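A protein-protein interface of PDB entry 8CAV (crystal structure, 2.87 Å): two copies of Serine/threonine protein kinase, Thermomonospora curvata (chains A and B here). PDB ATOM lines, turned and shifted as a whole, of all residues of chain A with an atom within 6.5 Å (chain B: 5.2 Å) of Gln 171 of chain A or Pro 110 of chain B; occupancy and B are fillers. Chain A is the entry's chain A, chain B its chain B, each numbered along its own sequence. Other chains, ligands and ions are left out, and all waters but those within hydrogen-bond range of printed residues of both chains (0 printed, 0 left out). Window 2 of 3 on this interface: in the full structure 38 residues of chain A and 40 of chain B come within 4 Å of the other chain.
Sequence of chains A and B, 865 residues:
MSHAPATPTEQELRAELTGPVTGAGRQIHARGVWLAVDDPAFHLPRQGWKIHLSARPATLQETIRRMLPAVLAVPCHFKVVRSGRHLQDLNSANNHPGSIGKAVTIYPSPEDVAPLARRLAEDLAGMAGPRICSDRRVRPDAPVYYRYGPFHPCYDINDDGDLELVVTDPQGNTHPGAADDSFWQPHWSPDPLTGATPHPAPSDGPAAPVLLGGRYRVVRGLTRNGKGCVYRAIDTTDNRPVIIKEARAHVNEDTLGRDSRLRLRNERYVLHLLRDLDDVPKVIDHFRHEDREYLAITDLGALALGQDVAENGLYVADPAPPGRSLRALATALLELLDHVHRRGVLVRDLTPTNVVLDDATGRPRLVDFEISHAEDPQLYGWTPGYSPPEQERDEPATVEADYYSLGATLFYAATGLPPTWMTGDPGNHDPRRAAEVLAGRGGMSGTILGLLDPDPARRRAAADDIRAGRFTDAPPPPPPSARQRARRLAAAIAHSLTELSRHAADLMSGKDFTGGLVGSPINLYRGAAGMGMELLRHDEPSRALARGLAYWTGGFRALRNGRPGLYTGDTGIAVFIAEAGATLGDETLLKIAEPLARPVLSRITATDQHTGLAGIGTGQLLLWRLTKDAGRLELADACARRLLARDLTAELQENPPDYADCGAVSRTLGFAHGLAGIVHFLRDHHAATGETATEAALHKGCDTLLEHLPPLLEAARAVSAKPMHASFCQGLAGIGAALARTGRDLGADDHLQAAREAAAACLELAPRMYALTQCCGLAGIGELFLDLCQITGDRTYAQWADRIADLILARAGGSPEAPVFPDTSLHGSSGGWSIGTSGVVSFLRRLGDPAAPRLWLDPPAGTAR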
ATOM      1  N   THR A 168       6.485  -7.803 -14.526  1.00  0.00           N
ATOM      2  CA  THR A 168       5.273  -7.876 -13.721  1.00  0.00           C
ATOM      3  C   THR A 168       4.466  -9.121 -14.060  1.00  0.00           C
ATOM      4  O   THR A 168       4.302  -9.465 -15.235  1.00  0.00           O
ATOM      5  CB  THR A 168       4.406  -6.632 -13.939  1.00  0.00           C
ATOM      6  OG1 THR A 168       5.208  -5.452 -13.798  1.00  0.00           O
ATOM      7  CG2 THR A 168       3.276  -6.593 -12.934  1.00  0.00           C
ATOM      8  N   ASP A 169       3.946  -9.784 -13.030  1.00  0.00           N
ATOM      9  CA  ASP A 169       3.123 -10.974 -13.208  1.00  0.00           C
ATOM     10  C   ASP A 169       1.658 -10.590 -13.323  1.00  0.00           C
ATOM     11  O   ASP A 169       1.274  -9.438 -13.110  1.00  0.00           O
ATOM     12  CB  ASP A 169       3.363 -11.956 -12.055  1.00  0.00           C
ATOM     13  CG  ASP A 169       2.676 -11.552 -10.746  1.00  0.00           C
ATOM     14  OD1 ASP A 169       1.906 -10.568 -10.705  1.00  0.00           O
ATOM     15  OD2 ASP A 169       2.917 -12.248  -9.735  1.00  0.00           O
ATOM     16  N   PRO A 170       0.800 -11.551 -13.672  1.00  0.00           N
ATOM     17  CA  PRO A 170      -0.626 -11.234 -13.861  1.00  0.00           C
ATOM     18  C   PRO A 170      -1.305 -10.605 -12.654  1.00  0.00           C
ATOM     19  O   PRO A 170      -2.341  -9.951 -12.828  1.00  0.00           O
ATOM     20  CB  PRO A 170      -1.243 -12.600 -14.196  1.00  0.00           C
ATOM     21  CG  PRO A 170      -0.128 -13.374 -14.814  1.00  0.00           C
ATOM     22  CD  PRO A 170       1.158 -12.878 -14.206  1.00  0.00           C
ATOM     23  N   GLN A 171      -0.779 -10.786 -11.442  1.00  0.00           N
ATOM     24  CA  GLN A 171      -1.327 -10.139 -10.256  1.00  0.00           C
ATOM     25  C   GLN A 171      -0.578  -8.858  -9.903  1.00  0.00           C
ATOM     26  O   GLN A 171      -0.688  -8.369  -8.773  1.00  0.00           O
ATOM     27  CB  GLN A 171      -1.327 -11.113  -9.077  1.00  0.00           C
ATOM     28  CG  GLN A 171      -2.445 -12.146  -9.166  1.00  0.00           C
ATOM     29  CD  GLN A 171      -2.146 -13.420  -8.403  1.00  0.00           C
ATOM     30  OE1 GLN A 171      -2.229 -14.516  -8.957  1.00  0.00           O
ATOM     31  NE2 GLN A 171      -1.810 -13.286  -7.125  1.00  0.00           N
ATOM     32  N   GLY A 172       0.173  -8.303 -10.853  1.00  0.00           N
ATOM     33  CA  GLY A 172       0.838  -7.035 -10.636  1.00  0.00           C
ATOM     34  C   GLY A 172       2.019  -7.083  -9.698  1.00  0.00           C
ATOM     35  O   GLY A 172       2.391  -6.048  -9.137  1.00  0.00           O
ATOM     36  N   ASN A 173       2.625  -8.249  -9.512  1.00  0.00           N
ATOM     37  CA  ASN A 173       3.749  -8.411  -8.599  1.00  0.00           C
ATOM     38  C   ASN A 173       5.058  -8.294  -9.367  1.00  0.00           C
ATOM     39  O   ASN A 173       5.254  -8.976 -10.380  1.00  0.00           O
ATOM     40  CB  ASN A 173       3.678  -9.757  -7.879  1.00  0.00           C
ATOM     41  CG  ASN A 173       2.426  -9.901  -7.035  1.00  0.00           C
ATOM     42  OD1 ASN A 173       1.923  -8.926  -6.477  1.00  0.00           O
ATOM     43  ND2 ASN A 173       1.916 -11.124  -6.938  1.00  0.00           N
ATOM     44  N   PRO B  45      -1.346  -9.251  -2.942  1.00  0.00           N
ATOM     45  CA  PRO B  45      -0.880  -8.917  -4.299  1.00  0.00           C
ATOM     46  C   PRO B  45      -1.215  -7.460  -4.596  1.00  0.00           C
ATOM     47  O   PRO B  45      -1.873  -6.781  -3.819  1.00  0.00           O
ATOM     48  CB  PRO B  45      -1.638  -9.892  -5.199  1.00  0.00           C
ATOM     49  CG  PRO B  45      -2.854 -10.262  -4.427  1.00  0.00           C
ATOM     50  CD  PRO B  45      -2.443 -10.245  -2.975  1.00  0.00           C
ATOM     51  N   ARG B  46      -0.746  -6.967  -5.753  1.00  0.00           N
ATOM     52  CA  ARG B  46      -0.871  -5.538  -6.044  1.00  0.00           C
ATOM     53  C   ARG B  46      -2.160  -5.182  -6.776  1.00  0.00           C
ATOM     54  O   ARG B  46      -2.538  -4.005  -6.805  1.00  0.00           O
ATOM     55  CB  ARG B  46       0.334  -5.066  -6.865  1.00  0.00           C
ATOM     56  CG  ARG B  46       0.695  -3.599  -6.672  1.00  0.00           C
ATOM     57  CD  ARG B  46       1.574  -3.353  -5.443  1.00  0.00           C
ATOM     58  NE  ARG B  46       2.810  -4.133  -5.433  1.00  0.00           N
ATOM     59  CZ  ARG B  46       3.826  -3.956  -6.268  1.00  0.00           C
ATOM     60  NH1 ARG B  46       3.757  -3.095  -7.271  1.00  0.00           N
ATOM     61  NH2 ARG B  46       4.939  -4.663  -6.093  1.00  0.00           N
ATOM     62  N   GLN B  47      -2.842  -6.165  -7.356  1.00  0.00           N
ATOM     63  CA  GLN B  47      -4.106  -5.942  -8.043  1.00  0.00           C
ATOM     64  C   GLN B  47      -4.844  -7.272  -8.079  1.00  0.00           C
ATOM     65  O   GLN B  47      -4.264  -8.328  -7.818  1.00  0.00           O
ATOM     66  CB  GLN B  47      -3.891  -5.411  -9.460  1.00  0.00           C
ATOM     67  CG  GLN B  47      -3.312  -6.463 -10.391  1.00  0.00           C
ATOM     68  CD  GLN B  47      -2.732  -5.887 -11.663  1.00  0.00           C
ATOM     69  OE1 GLN B  47      -2.296  -4.736 -11.701  1.00  0.00           O
ATOM     70  NE2 GLN B  47      -2.719  -6.691 -12.719  1.00  0.00           N
ATOM     71  N   PRO B 108      -8.612 -11.150  -0.897  1.00  0.00           N
ATOM     72  CA  PRO B 108      -8.177 -12.515  -0.580  1.00  0.00           C
ATOM     73  C   PRO B 108      -7.340 -13.121  -1.689  1.00  0.00           C
ATOM     74  O   PRO B 108      -7.102 -12.477  -2.720  1.00  0.00           O
ATOM     75  CB  PRO B 108      -9.511 -13.254  -0.414  1.00  0.00           C
ATOM     76  CG  PRO B 108     -10.494 -12.463  -1.332  1.00  0.00           C
ATOM     77  CD  PRO B 108      -9.776 -11.192  -1.793  1.00  0.00           C
ATOM     78  N   SER B 109      -6.893 -14.359  -1.500  1.00  0.00           N
ATOM     79  CA  SER B 109      -6.126 -15.030  -2.540  1.00  0.00           C
ATOM     80  C   SER B 109      -7.049 -15.425  -3.692  1.00  0.00           C
ATOM     81  O   SER B 109      -8.177 -15.874  -3.455  1.00  0.00           O
ATOM     82  CB  SER B 109      -5.422 -16.265  -1.978  1.00  0.00           C
ATOM     83  OG  SER B 109      -4.295 -15.897  -1.199  1.00  0.00           O
ATOM     84  N   PRO B 110      -6.601 -15.262  -4.949  1.00  0.00           N
ATOM     85  CA  PRO B 110      -7.460 -15.593  -6.098  1.00  0.00           C
ATOM     86  C   PRO B 110      -8.190 -16.916  -5.931  1.00  0.00           C
ATOM     87  O   PRO B 110      -9.420 -16.985  -6.008  1.00  0.00           O
ATOM     88  CB  PRO B 110      -6.465 -15.650  -7.267  1.00  0.00           C
ATOM     89  CG  PRO B 110      -5.363 -14.726  -6.862  1.00  0.00           C
ATOM     90  CD  PRO B 110      -5.263 -14.796  -5.363  1.00  0.00           C
ATOM     91  N   GLU B 111      -7.415 -17.971  -5.703  1.00  0.00           N
ATOM     92  CA  GLU B 111      -7.919 -19.289  -5.350  1.00  0.00           C
ATOM     93  C   GLU B 111      -9.121 -19.253  -4.413  1.00  0.00           C
ATOM     94  O   GLU B 111     -10.024 -20.089  -4.535  1.00  0.00           O
ATOM     95  CB  GLU B 111      -6.770 -20.093  -4.718  1.00  0.00           C
ATOM     96  CG  GLU B 111      -5.938 -19.301  -3.697  1.00  0.00           C
ATOM     97  CD  GLU B 111      -4.528 -19.845  -3.530  1.00  0.00           C
ATOM     98  OE1 GLU B 111      -3.717 -19.697  -4.470  1.00  0.00           O
ATOM     99  OE2 GLU B 111      -4.234 -20.422  -2.460  1.00  0.00           O
ATOM    100  N   ASP B 112      -9.159 -18.293  -3.492  1.00  0.00           N
ATOM    101  CA  ASP B 112     -10.191 -18.245  -2.462  1.00  0.00           C
ATOM    102  C   ASP B 112     -11.281 -17.211  -2.721  1.00  0.00           C
ATOM    103  O   ASP B 112     -12.199 -17.090  -1.904  1.00  0.00           O
ATOM    104  CB  ASP B 112      -9.552 -17.959  -1.093  1.00  0.00           C
ATOM    105  CG  ASP B 112      -8.806 -19.154  -0.530  1.00  0.00           C
ATOM    106  OD1 ASP B 112      -9.257 -20.299  -0.754  1.00  0.00           O
ATOM    107  OD2 ASP B 112      -7.774 -18.945   0.143  1.00  0.00           O
ATOM    108  N   VAL B 113     -11.221 -16.470  -3.824  1.00  0.00           N
ATOM    109  CA  VAL B 113     -12.149 -15.363  -4.040  1.00  0.00           C
ATOM    110  C   VAL B 113     -13.567 -15.875  -4.263  1.00  0.00           C
ATOM    111  O   VAL B 113     -14.453 -15.632  -3.436  1.00  0.00           O
ATOM    112  CB  VAL B 113     -11.688 -14.477  -5.213  1.00  0.00           C
ATOM    113  CG1 VAL B 113     -12.848 -13.659  -5.769  1.00  0.00           C
ATOM    114  CG2 VAL B 113     -10.572 -13.553  -4.751  1.00  0.00           C
ATOM    115  N   ALA B 114     -13.802 -16.569  -5.379  1.00  0.00           N
ATOM    116  CA  ALA B 114     -15.144 -17.071  -5.674  1.00  0.00           C
ATOM    117  C   ALA B 114     -15.788 -17.768  -4.484  1.00  0.00           C
ATOM    118  O   ALA B 114     -16.931 -17.425  -4.141  1.00  0.00           O
ATOM    119  CB  ALA B 114     -15.087 -18.008  -6.889  1.00  0.00           C
ATOM    120  N   TYR B 148     -12.514  -6.231 -10.243  1.00  0.00           N
ATOM    121  CA  TYR B 148     -11.070  -6.272 -10.450  1.00  0.00           C
ATOM    122  C   TYR B 148     -10.537  -4.847 -10.394  1.00  0.00           C
ATOM    123  O   TYR B 148     -11.038  -3.963 -11.098  1.00  0.00           O
ATOM    124  CB  TYR B 148     -10.706  -6.912 -11.792  1.00  0.00           C
ATOM    125  CG  TYR B 148      -9.253  -7.355 -11.929  1.00  0.00           C
ATOM    126  CD1 TYR B 148      -8.236  -6.438 -12.179  1.00  0.00           C
ATOM    127  CD2 TYR B 148      -8.908  -8.698 -11.839  1.00  0.00           C
ATOM    128  CE1 TYR B 148      -6.914  -6.848 -12.317  1.00  0.00           C
ATOM    129  CE2 TYR B 148      -7.595  -9.115 -11.979  1.00  0.00           C
ATOM    130  CZ  TYR B 148      -6.603  -8.187 -12.215  1.00  0.00           C
ATOM    131  OH  TYR B 148      -5.296  -8.601 -12.350  1.00  0.00           O
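Of the 11 printed residues of chain B, 5 touch a printed residue of chain A.
Printed residues of chain B that touch a printed residue of chain A: Pro 45, Arg 46, Gln 47, Pro 110 and Tyr 148.
Hydrophobic or aromatic side chains of chain B within 4 Å of the printed part of chain A: Pro 45, Pro 110 and Tyr 148.
Among the printed residues, 10 pairs touch across the chains.
Among the printed residues, merely in contact across the chains: Gly 172 of chain A with Arg 46 of chain B, Asn 173 of chain A with Pro 45 of chain B, Gln 171 of chain A with Pro 110 of chain B, Gly 172 of chain A with Gln 47 of chain B and Gln 171 of chain A with Pro 45 of chain B.
No position is printed for both chains.
Of the 10 pairs that touch across the chains among the printed residues, none has its exchanged pair printed and touching as well.
Printed residues of chain B within 4 Å of Pro 170 of chain A: Gln 47 (3.3 Å) and Tyr 148 (3.3 Å).
Gln 171 of chain A touches just these residues of chain B: Pro 45 (3.9 Å), Arg 46 (3.3 Å), Gln 47 (3.4 Å) and Pro 110 (3.8 Å).
Of the printed residues of chain A, Pro 45 of chain B touches Gln 171 and Asn 173.
Pro 110 of chain B touches one residue of chain A.
Val 113 of chain B touches none of the printed residues of chain A.
Of the printed residues of chain A, Tyr 148 of chain B touches Pro 170.
The backbone carbonyl oxygen (O) of Pro 170 of chain A lies within hydrogen-bond range of the side-chain amide nitrogen (NE2) of Gln 47 of chain B (3.3 Å).
O of Pro 170 of chain A lies within hydrogen-bond range of OH of Tyr 148 of chain B, at 3.3 Å.
The backbone carbonyl oxygen (O) of Gln 171 of chain A sits at hydrogen-bond distance from the backbone NH (N) of Arg 46 of chain B, at 3.3 Å.
O of Gln 171 of chain A is in hydrogen-bond range of N of Gln 47 of chain B (3.4 Å).
The side-chain amide oxygen of Asn 173 of chain A sits at hydrogen-bond distance from the backbone NH of Arg 46 of chain B.
The side-chain carboxylate (OD1) of Asp 169 of chain A is in hydrogen-bond range of the backbone NH (N) of Gln 171 of chain A, 2.8 Å away.
The backbone NH (N) of Gly 172 of chain A is in hydrogen-bond range of the side-chain carboxylate (OD1) of Asp 169 of chain A, 2.9 Å away.
The backbone NH (N) of Asn 173 of chain A sits at hydrogen-bond distance from the side-chain carboxylate (OD1) of Asp 169 of chain A, 2.7 Å away.
The side-chain hydroxyl (OH) of Tyr 148 of chain B sits at hydrogen-bond distance from the side-chain amide nitrogen (NE2) of Gln 47 of chain B, at 3.2 Å.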
